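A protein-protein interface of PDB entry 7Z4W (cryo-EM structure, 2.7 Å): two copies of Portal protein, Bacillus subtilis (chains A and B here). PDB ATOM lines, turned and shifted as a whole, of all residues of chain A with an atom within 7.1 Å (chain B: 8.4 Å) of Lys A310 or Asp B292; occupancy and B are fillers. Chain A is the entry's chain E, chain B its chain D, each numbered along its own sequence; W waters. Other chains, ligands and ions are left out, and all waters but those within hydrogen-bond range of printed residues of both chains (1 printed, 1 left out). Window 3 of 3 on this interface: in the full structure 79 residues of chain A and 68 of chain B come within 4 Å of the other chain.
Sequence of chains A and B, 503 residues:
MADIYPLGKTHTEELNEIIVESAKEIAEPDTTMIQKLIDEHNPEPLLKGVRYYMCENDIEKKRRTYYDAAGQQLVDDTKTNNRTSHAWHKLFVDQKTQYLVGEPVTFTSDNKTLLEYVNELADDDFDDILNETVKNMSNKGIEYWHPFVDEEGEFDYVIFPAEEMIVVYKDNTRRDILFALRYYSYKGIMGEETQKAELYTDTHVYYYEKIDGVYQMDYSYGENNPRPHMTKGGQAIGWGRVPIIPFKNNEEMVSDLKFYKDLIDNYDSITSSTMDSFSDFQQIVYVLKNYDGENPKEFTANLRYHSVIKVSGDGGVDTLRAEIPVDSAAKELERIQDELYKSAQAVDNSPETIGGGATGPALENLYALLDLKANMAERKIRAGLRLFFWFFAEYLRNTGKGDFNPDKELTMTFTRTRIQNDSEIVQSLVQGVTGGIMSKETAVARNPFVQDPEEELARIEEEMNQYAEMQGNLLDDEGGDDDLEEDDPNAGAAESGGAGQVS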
ATOM      1  N   TYR A 291     -38.439  14.885  -3.377  1.00  0.00           N
ATOM      2  CA  TYR A 291     -37.410  15.524  -4.209  1.00  0.00           C
ATOM      3  C   TYR A 291     -37.802  15.322  -5.673  1.00  0.00           C
ATOM      4  O   TYR A 291     -37.302  14.427  -6.350  1.00  0.00           O
ATOM      5  CB  TYR A 291     -36.019  14.955  -3.924  1.00  0.00           C
ATOM      6  CG  TYR A 291     -35.449  15.351  -2.587  1.00  0.00           C
ATOM      7  CD1 TYR A 291     -35.002  16.646  -2.358  1.00  0.00           C
ATOM      8  CD2 TYR A 291     -35.363  14.429  -1.549  1.00  0.00           C
ATOM      9  CE1 TYR A 291     -34.487  17.011  -1.139  1.00  0.00           C
ATOM     10  CE2 TYR A 291     -34.847  14.787  -0.328  1.00  0.00           C
ATOM     11  CZ  TYR A 291     -34.412  16.078  -0.127  1.00  0.00           C
ATOM     12  OH  TYR A 291     -33.898  16.442   1.089  1.00  0.00           O
ATOM     13  N   VAL A 308     -22.284   9.309   0.637  1.00  0.00           N
ATOM     14  CA  VAL A 308     -23.005  10.148   1.591  1.00  0.00           C
ATOM     15  C   VAL A 308     -24.236  10.709   0.882  1.00  0.00           C
ATOM     16  O   VAL A 308     -24.144  11.142  -0.271  1.00  0.00           O
ATOM     17  CB  VAL A 308     -22.113  11.291   2.138  1.00  0.00           C
ATOM     18  CG1 VAL A 308     -22.906  12.296   2.963  1.00  0.00           C
ATOM     19  CG2 VAL A 308     -20.975  10.752   2.982  1.00  0.00           C
ATOM     20  N   ILE A 309     -25.388  10.678   1.557  1.00  0.00           N
ATOM     21  CA  ILE A 309     -26.624  11.285   1.073  1.00  0.00           C
ATOM     22  C   ILE A 309     -27.066  12.339   2.085  1.00  0.00           C
ATOM     23  O   ILE A 309     -27.071  12.080   3.292  1.00  0.00           O
ATOM     24  CB  ILE A 309     -27.722  10.217   0.868  1.00  0.00           C
ATOM     25  CG1 ILE A 309     -27.366   9.291  -0.289  1.00  0.00           C
ATOM     26  CG2 ILE A 309     -29.083  10.839   0.586  1.00  0.00           C
ATOM     27  CD1 ILE A 309     -28.113   7.987  -0.236  1.00  0.00           C
ATOM     28  N   LYS A 310     -27.431  13.525   1.596  1.00  0.00           N
ATOM     29  CA  LYS A 310     -27.923  14.619   2.428  1.00  0.00           C
ATOM     30  C   LYS A 310     -29.416  14.830   2.203  1.00  0.00           C
ATOM     31  O   LYS A 310     -29.846  15.063   1.071  1.00  0.00           O
ATOM     32  CB  LYS A 310     -27.174  15.916   2.128  1.00  0.00           C
ATOM     33  CG  LYS A 310     -25.675  15.828   2.266  1.00  0.00           C
ATOM     34  CD  LYS A 310     -25.083  17.197   2.524  1.00  0.00           C
ATOM     35  CE  LYS A 310     -24.213  17.646   1.375  1.00  0.00           C
ATOM     36  NZ  LYS A 310     -23.928  19.100   1.435  1.00  0.00           N
ATOM     37  N   VAL A 311     -30.199  14.758   3.280  1.00  0.00           N
ATOM     38  CA  VAL A 311     -31.632  15.038   3.254  1.00  0.00           C
ATOM     39  C   VAL A 311     -31.952  16.047   4.351  1.00  0.00           C
ATOM     40  O   VAL A 311     -31.207  16.169   5.328  1.00  0.00           O
ATOM     41  CB  VAL A 311     -32.489  13.761   3.429  1.00  0.00           C
ATOM     42  CG1 VAL A 311     -32.318  12.818   2.246  1.00  0.00           C
ATOM     43  CG2 VAL A 311     -32.178  13.060   4.742  1.00  0.00           C
ATOM     44  N   SER A 312     -33.041  16.796   4.175  1.00  0.00           N
ATOM     45  CA  SER A 312     -33.506  17.738   5.187  1.00  0.00           C
ATOM     46  C   SER A 312     -35.013  17.926   5.078  1.00  0.00           C
ATOM     47  O   SER A 312     -35.601  17.753   4.009  1.00  0.00           O
ATOM     48  CB  SER A 312     -32.806  19.099   5.065  1.00  0.00           C
ATOM     49  OG  SER A 312     -32.863  19.583   3.740  1.00  0.00           O
ATOM     50  N   GLY A 313     -35.632  18.273   6.202  1.00  0.00           N
ATOM     51  CA  GLY A 313     -37.038  18.663   6.188  1.00  0.00           C
ATOM     52  C   GLY A 313     -37.950  17.463   6.119  1.00  0.00           C
ATOM     53  O   GLY A 313     -37.853  16.548   6.932  1.00  0.00           O
ATOM     54  N   VAL A 317     -35.115   9.202   1.984  1.00  0.00           N
ATOM     55  CA  VAL A 317     -34.630   8.188   1.055  1.00  0.00           C
ATOM     56  C   VAL A 317     -34.796   6.822   1.714  1.00  0.00           C
ATOM     57  O   VAL A 317     -34.607   6.671   2.923  1.00  0.00           O
ATOM     58  CB  VAL A 317     -33.173   8.488   0.611  1.00  0.00           C
ATOM     59  CG1 VAL A 317     -32.203   8.518   1.793  1.00  0.00           C
ATOM     60  CG2 VAL A 317     -32.702   7.519  -0.470  1.00  0.00           C
ATOM     61  N   TYR B 286     -23.846   6.413   4.171  1.00  0.00           N
ATOM     62  CA  TYR B 286     -24.221   7.293   5.274  1.00  0.00           C
ATOM     63  C   TYR B 286     -25.331   8.240   4.832  1.00  0.00           C
ATOM     64  O   TYR B 286     -25.357   8.684   3.683  1.00  0.00           O
ATOM     65  CB  TYR B 286     -23.028   8.125   5.758  1.00  0.00           C
ATOM     66  CG  TYR B 286     -21.891   7.354   6.380  1.00  0.00           C
ATOM     67  CD1 TYR B 286     -22.045   6.710   7.599  1.00  0.00           C
ATOM     68  CD2 TYR B 286     -20.650   7.292   5.756  1.00  0.00           C
ATOM     69  CE1 TYR B 286     -21.001   6.010   8.171  1.00  0.00           C
ATOM     70  CE2 TYR B 286     -19.604   6.599   6.320  1.00  0.00           C
ATOM     71  CZ  TYR B 286     -19.784   5.958   7.524  1.00  0.00           C
ATOM     72  OH  TYR B 286     -18.745   5.263   8.083  1.00  0.00           O
ATOM     73  N   VAL B 287     -26.243   8.554   5.749  1.00  0.00           N
ATOM     74  CA  VAL B 287     -27.320   9.513   5.508  1.00  0.00           C
ATOM     75  C   VAL B 287     -27.214  10.627   6.542  1.00  0.00           C
ATOM     76  O   VAL B 287     -27.296  10.369   7.749  1.00  0.00           O
ATOM     77  CB  VAL B 287     -28.710   8.856   5.565  1.00  0.00           C
ATOM     78  CG1 VAL B 287     -29.773   9.836   5.105  1.00  0.00           C
ATOM     79  CG2 VAL B 287     -28.761   7.590   4.722  1.00  0.00           C
ATOM     80  N   LEU B 288     -27.038  11.859   6.071  1.00  0.00           N
ATOM     81  CA  LEU B 288     -27.019  13.046   6.918  1.00  0.00           C
ATOM     82  C   LEU B 288     -28.383  13.726   6.903  1.00  0.00           C
ATOM     83  O   LEU B 288     -29.000  13.873   5.846  1.00  0.00           O
ATOM     84  CB  LEU B 288     -25.951  14.036   6.449  1.00  0.00           C
ATOM     85  CG  LEU B 288     -24.484  13.719   6.731  1.00  0.00           C
ATOM     86  CD1 LEU B 288     -23.589  14.772   6.113  1.00  0.00           C
ATOM     87  CD2 LEU B 288     -24.232  13.618   8.222  1.00  0.00           C
ATOM     88  N   LYS B 289     -28.844  14.151   8.077  1.00  0.00           N
ATOM     89  CA  LYS B 289     -30.139  14.802   8.241  1.00  0.00           C
ATOM     90  C   LYS B 289     -29.923  16.214   8.765  1.00  0.00           C
ATOM     91  O   LYS B 289     -29.343  16.391   9.845  1.00  0.00           O
ATOM     92  CB  LYS B 289     -31.035  14.011   9.194  1.00  0.00           C
ATOM     93  CG  LYS B 289     -31.814  12.905   8.527  1.00  0.00           C
ATOM     94  CD  LYS B 289     -32.065  11.747   9.475  1.00  0.00           C
ATOM     95  CE  LYS B 289     -30.775  11.018   9.836  1.00  0.00           C
ATOM     96  NZ  LYS B 289     -30.076  10.490   8.639  1.00  0.00           N
ATOM     97  N   ASN B 290     -30.382  17.200   7.982  1.00  0.00           N
ATOM     98  CA  ASN B 290     -30.384  18.635   8.313  1.00  0.00           C
ATOM     99  C   ASN B 290     -28.971  19.195   8.480  1.00  0.00           C
ATOM    100  O   ASN B 290     -28.712  20.014   9.359  1.00  0.00           O
ATOM    101  CB  ASN B 290     -31.242  18.937   9.549  1.00  0.00           C
ATOM    102  CG  ASN B 290     -32.706  18.616   9.339  1.00  0.00           C
ATOM    103  OD1 ASN B 290     -33.338  19.137   8.430  1.00  0.00           O
ATOM    104  ND2 ASN B 290     -33.249  17.752  10.179  1.00  0.00           N
ATOM    105  N   TYR B 291     -28.043  18.745   7.631  1.00  0.00           N
ATOM    106  CA  TYR B 291     -26.714  19.349   7.508  1.00  0.00           C
ATOM    107  C   TYR B 291     -26.438  19.556   6.020  1.00  0.00           C
ATOM    108  O   TYR B 291     -25.722  18.775   5.399  1.00  0.00           O
ATOM    109  CB  TYR B 291     -25.651  18.467   8.164  1.00  0.00           C
ATOM    110  CG  TYR B 291     -25.672  18.506   9.670  1.00  0.00           C
ATOM    111  CD1 TYR B 291     -25.316  19.662  10.355  1.00  0.00           C
ATOM    112  CD2 TYR B 291     -26.059  17.396  10.409  1.00  0.00           C
ATOM    113  CE1 TYR B 291     -25.341  19.709  11.727  1.00  0.00           C
ATOM    114  CE2 TYR B 291     -26.085  17.435  11.784  1.00  0.00           C
ATOM    115  CZ  TYR B 291     -25.725  18.594  12.436  1.00  0.00           C
ATOM    116  OH  TYR B 291     -25.749  18.644  13.806  1.00  0.00           O
ATOM    117  N   ASP B 292     -26.950  20.648   5.463  1.00  0.00           N
ATOM    118  CA  ASP B 292     -26.920  20.836   4.019  1.00  0.00           C
ATOM    119  C   ASP B 292     -25.700  21.600   3.528  1.00  0.00           C
ATOM    120  O   ASP B 292     -25.431  21.584   2.324  1.00  0.00           O
ATOM    121  CB  ASP B 292     -28.188  21.551   3.551  1.00  0.00           C
ATOM    122  CG  ASP B 292     -29.348  20.601   3.333  1.00  0.00           C
ATOM    123  OD1 ASP B 292     -29.145  19.372   3.394  1.00  0.00           O
ATOM    124  OD2 ASP B 292     -30.472  21.085   3.100  1.00  0.00           O
ATOM    125  N   GLY B 293     -24.961  22.259   4.412  1.00  0.00           N
ATOM    126  CA  GLY B 293     -23.735  22.927   4.042  1.00  0.00           C
ATOM    127  C   GLY B 293     -22.470  22.116   4.203  1.00  0.00           C
ATOM    128  O   GLY B 293     -21.382  22.638   3.949  1.00  0.00           O
ATOM    129  N   GLU B 294     -22.573  20.851   4.595  1.00  0.00           N
ATOM    130  CA  GLU B 294     -21.407  20.041   4.929  1.00  0.00           C
ATOM    131  C   GLU B 294     -20.737  19.474   3.677  1.00  0.00           C
ATOM    132  O   GLU B 294     -21.409  18.973   2.772  1.00  0.00           O
ATOM    133  CB  GLU B 294     -21.826  18.912   5.875  1.00  0.00           C
ATOM    134  CG  GLU B 294     -20.742  17.911   6.215  1.00  0.00           C
ATOM    135  CD  GLU B 294     -19.845  18.373   7.343  1.00  0.00           C
ATOM    136  OE1 GLU B 294     -20.194  19.358   8.022  1.00  0.00           O
ATOM    137  OE2 GLU B 294     -18.781  17.757   7.544  1.00  0.00           O
ATOM    138  N   ASN B 295     -19.410  19.565   3.629  1.00  0.00           N
ATOM    139  CA  ASN B 295     -18.608  18.931   2.581  1.00  0.00           C
ATOM    140  C   ASN B 295     -18.501  17.429   2.836  1.00  0.00           C
ATOM    141  O   ASN B 295     -18.059  17.030   3.919  1.00  0.00           O
ATOM    142  CB  ASN B 295     -17.218  19.572   2.547  1.00  0.00           C
ATOM    143  CG  ASN B 295     -16.517  19.401   1.213  1.00  0.00           C
ATOM    144  OD1 ASN B 295     -16.564  18.343   0.596  1.00  0.00           O
ATOM    145  ND2 ASN B 295     -15.849  20.451   0.770  1.00  0.00           N
ATOM    146  N   PRO B 296     -18.897  16.571   1.885  1.00  0.00           N
ATOM    147  CA  PRO B 296     -18.873  15.114   2.139  1.00  0.00           C
ATOM    148  C   PRO B 296     -17.482  14.506   2.275  1.00  0.00           C
ATOM    149  O   PRO B 296     -17.295  13.593   3.094  1.00  0.00           O
ATOM    150  CB  PRO B 296     -19.618  14.540   0.923  1.00  0.00           C
ATOM    151  CG  PRO B 296     -20.405  15.668   0.380  1.00  0.00           C
ATOM    152  CD  PRO B 296     -19.604  16.897   0.637  1.00  0.00           C
ATOM    153  N   LYS B 297     -16.514  14.976   1.479  1.00  0.00           N
ATOM    154  CA  LYS B 297     -15.149  14.448   1.515  1.00  0.00           C
ATOM    155  C   LYS B 297     -14.491  14.690   2.870  1.00  0.00           C
ATOM    156  O   LYS B 297     -13.920  13.769   3.475  1.00  0.00           O
ATOM    157  CB  LYS B 297     -14.328  15.093   0.397  1.00  0.00           C
ATOM    158  CG  LYS B 297     -12.883  14.659   0.337  1.00  0.00           C
ATOM    159  CD  LYS B 297     -12.200  15.200  -0.901  1.00  0.00           C
ATOM    160  CE  LYS B 297     -11.968  16.692  -0.801  1.00  0.00           C
ATOM    161  NZ  LYS B 297     -10.951  17.007   0.233  1.00  0.00           N
ATOM    162  N   PHE B 299     -16.098  15.270   5.581  1.00  0.00           N
ATOM    163  CA  PHE B 299     -16.898  14.533   6.555  1.00  0.00           C
ATOM    164  C   PHE B 299     -16.411  13.093   6.709  1.00  0.00           C
ATOM    165  O   PHE B 299     -16.198  12.621   7.832  1.00  0.00           O
ATOM    166  CB  PHE B 299     -18.375  14.581   6.150  1.00  0.00           C
ATOM    167  CG  PHE B 299     -19.245  13.595   6.874  1.00  0.00           C
ATOM    168  CD1 PHE B 299     -19.604  13.811   8.193  1.00  0.00           C
ATOM    169  CD2 PHE B 299     -19.731  12.469   6.228  1.00  0.00           C
ATOM    170  CE1 PHE B 299     -20.404  12.912   8.865  1.00  0.00           C
ATOM    171  CE2 PHE B 299     -20.532  11.565   6.895  1.00  0.00           C
ATOM    172  CZ  PHE B 299     -20.873  11.792   8.212  1.00  0.00           C
ATOM    173  N   GLY B 316     -29.057  14.787  12.333  1.00  0.00           N
ATOM    174  CA  GLY B 316     -28.882  13.376  12.618  1.00  0.00           C
ATOM    175  C   GLY B 316     -28.010  12.694  11.592  1.00  0.00           C
ATOM    176  O   GLY B 316     -27.684  13.252  10.544  1.00  0.00           O
HETATM  177  O   HOH W   1     -30.569  17.962   0.716  1.00  0.00           O
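Of the 8 printed residues of chain A, 6 touch a printed residue of chain B.
Among the printed residues, no Asp or Glu carboxylate lies within 4 Å of a Lys or Arg side-chain nitrogen of the other chain.
Position printed for both chains: 291.
Of the 15 pairs that touch across the chains among the printed residues, none has its exchanged pair printed and touching as well.
The backbone carbonyl oxygen of Val B287 sits at hydrogen-bond distance from the side-chain amino group of Lys B289, 2.9 Å away.
N of Lys B289 lies within hydrogen-bond range of O of Gly B316 (2.9 Å).
The side-chain hydroxyl (OH) of Tyr A291 lies within hydrogen-bond range of the backbone NH (N) of Ser A312, 3.2 Å away.
Water W1 bridges the backbone carbonyl oxygen (O) of Lys A310 and the side-chain carboxylate (OD1) of Asp B292.
CA of Val A308 touches O of Tyr B286, at 3.5 Å.
Val A308 touches Phe B299.
Ile A309 touches Val B287.
Lys A310 touches Leu B288.
Lys A310 touches Tyr B291 (CD to O, 3.3 Å).
CA of Lys B289 touches O of Val A311, at 3.4 Å.
Ser A312 touches Asn B290 (CB to OD1, 3.4 Å).
Printed residues of chain B within 4 Å of Val A308: Tyr B286 and Phe B299.
Of the printed residues of chain A, Tyr B286 touches Val A308 and Ile A309.
Asp B292 touches just these residues of chain A: Lys A310 (3.0 Å) and Ser A312 (2.9 Å).
The nearest residue of chain B that does not touch Lys A310 is Gly B293 (4.3 Å).
The nearest printed residue of chain A that does not touch Val B287 is Val A311 (4.04 Å).
The backbone NH (N) of Ile A309 is in hydrogen-bond range of the backbone carbonyl oxygen (O) of Tyr B286, 2.9 Å away.
The backbone NH of Leu B288 sits at hydrogen-bond distance from the backbone carbonyl oxygen of Ile A309, at 2.8 Å.
The backbone NH (N) of Val A311 lies within hydrogen-bond range of the backbone carbonyl oxygen (O) of Leu B288 (3.0 Å).
The backbone NH of Asn B290 is in hydrogen-bond range of the backbone carbonyl oxygen of Val A311, at 3.0 Å.
The side-chain amide oxygen (OD1) of Asn B290 is in hydrogen-bond range of the backbone NH (N) of Gly A313 (3.3 Å).
NZ of Lys A310 sits at hydrogen-bond distance from O of Asp B292, 3.0 Å away.
The side-chain carboxylate (OD2) of Asp B292 lies within hydrogen-bond range of the side-chain hydroxyl (OG) of Ser A312 (2.9 Å).
The backbone carbonyl oxygen (O) of Glu B294 is in hydrogen-bond range of the side-chain amino group (NZ) of Lys A310 (2.9 Å).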
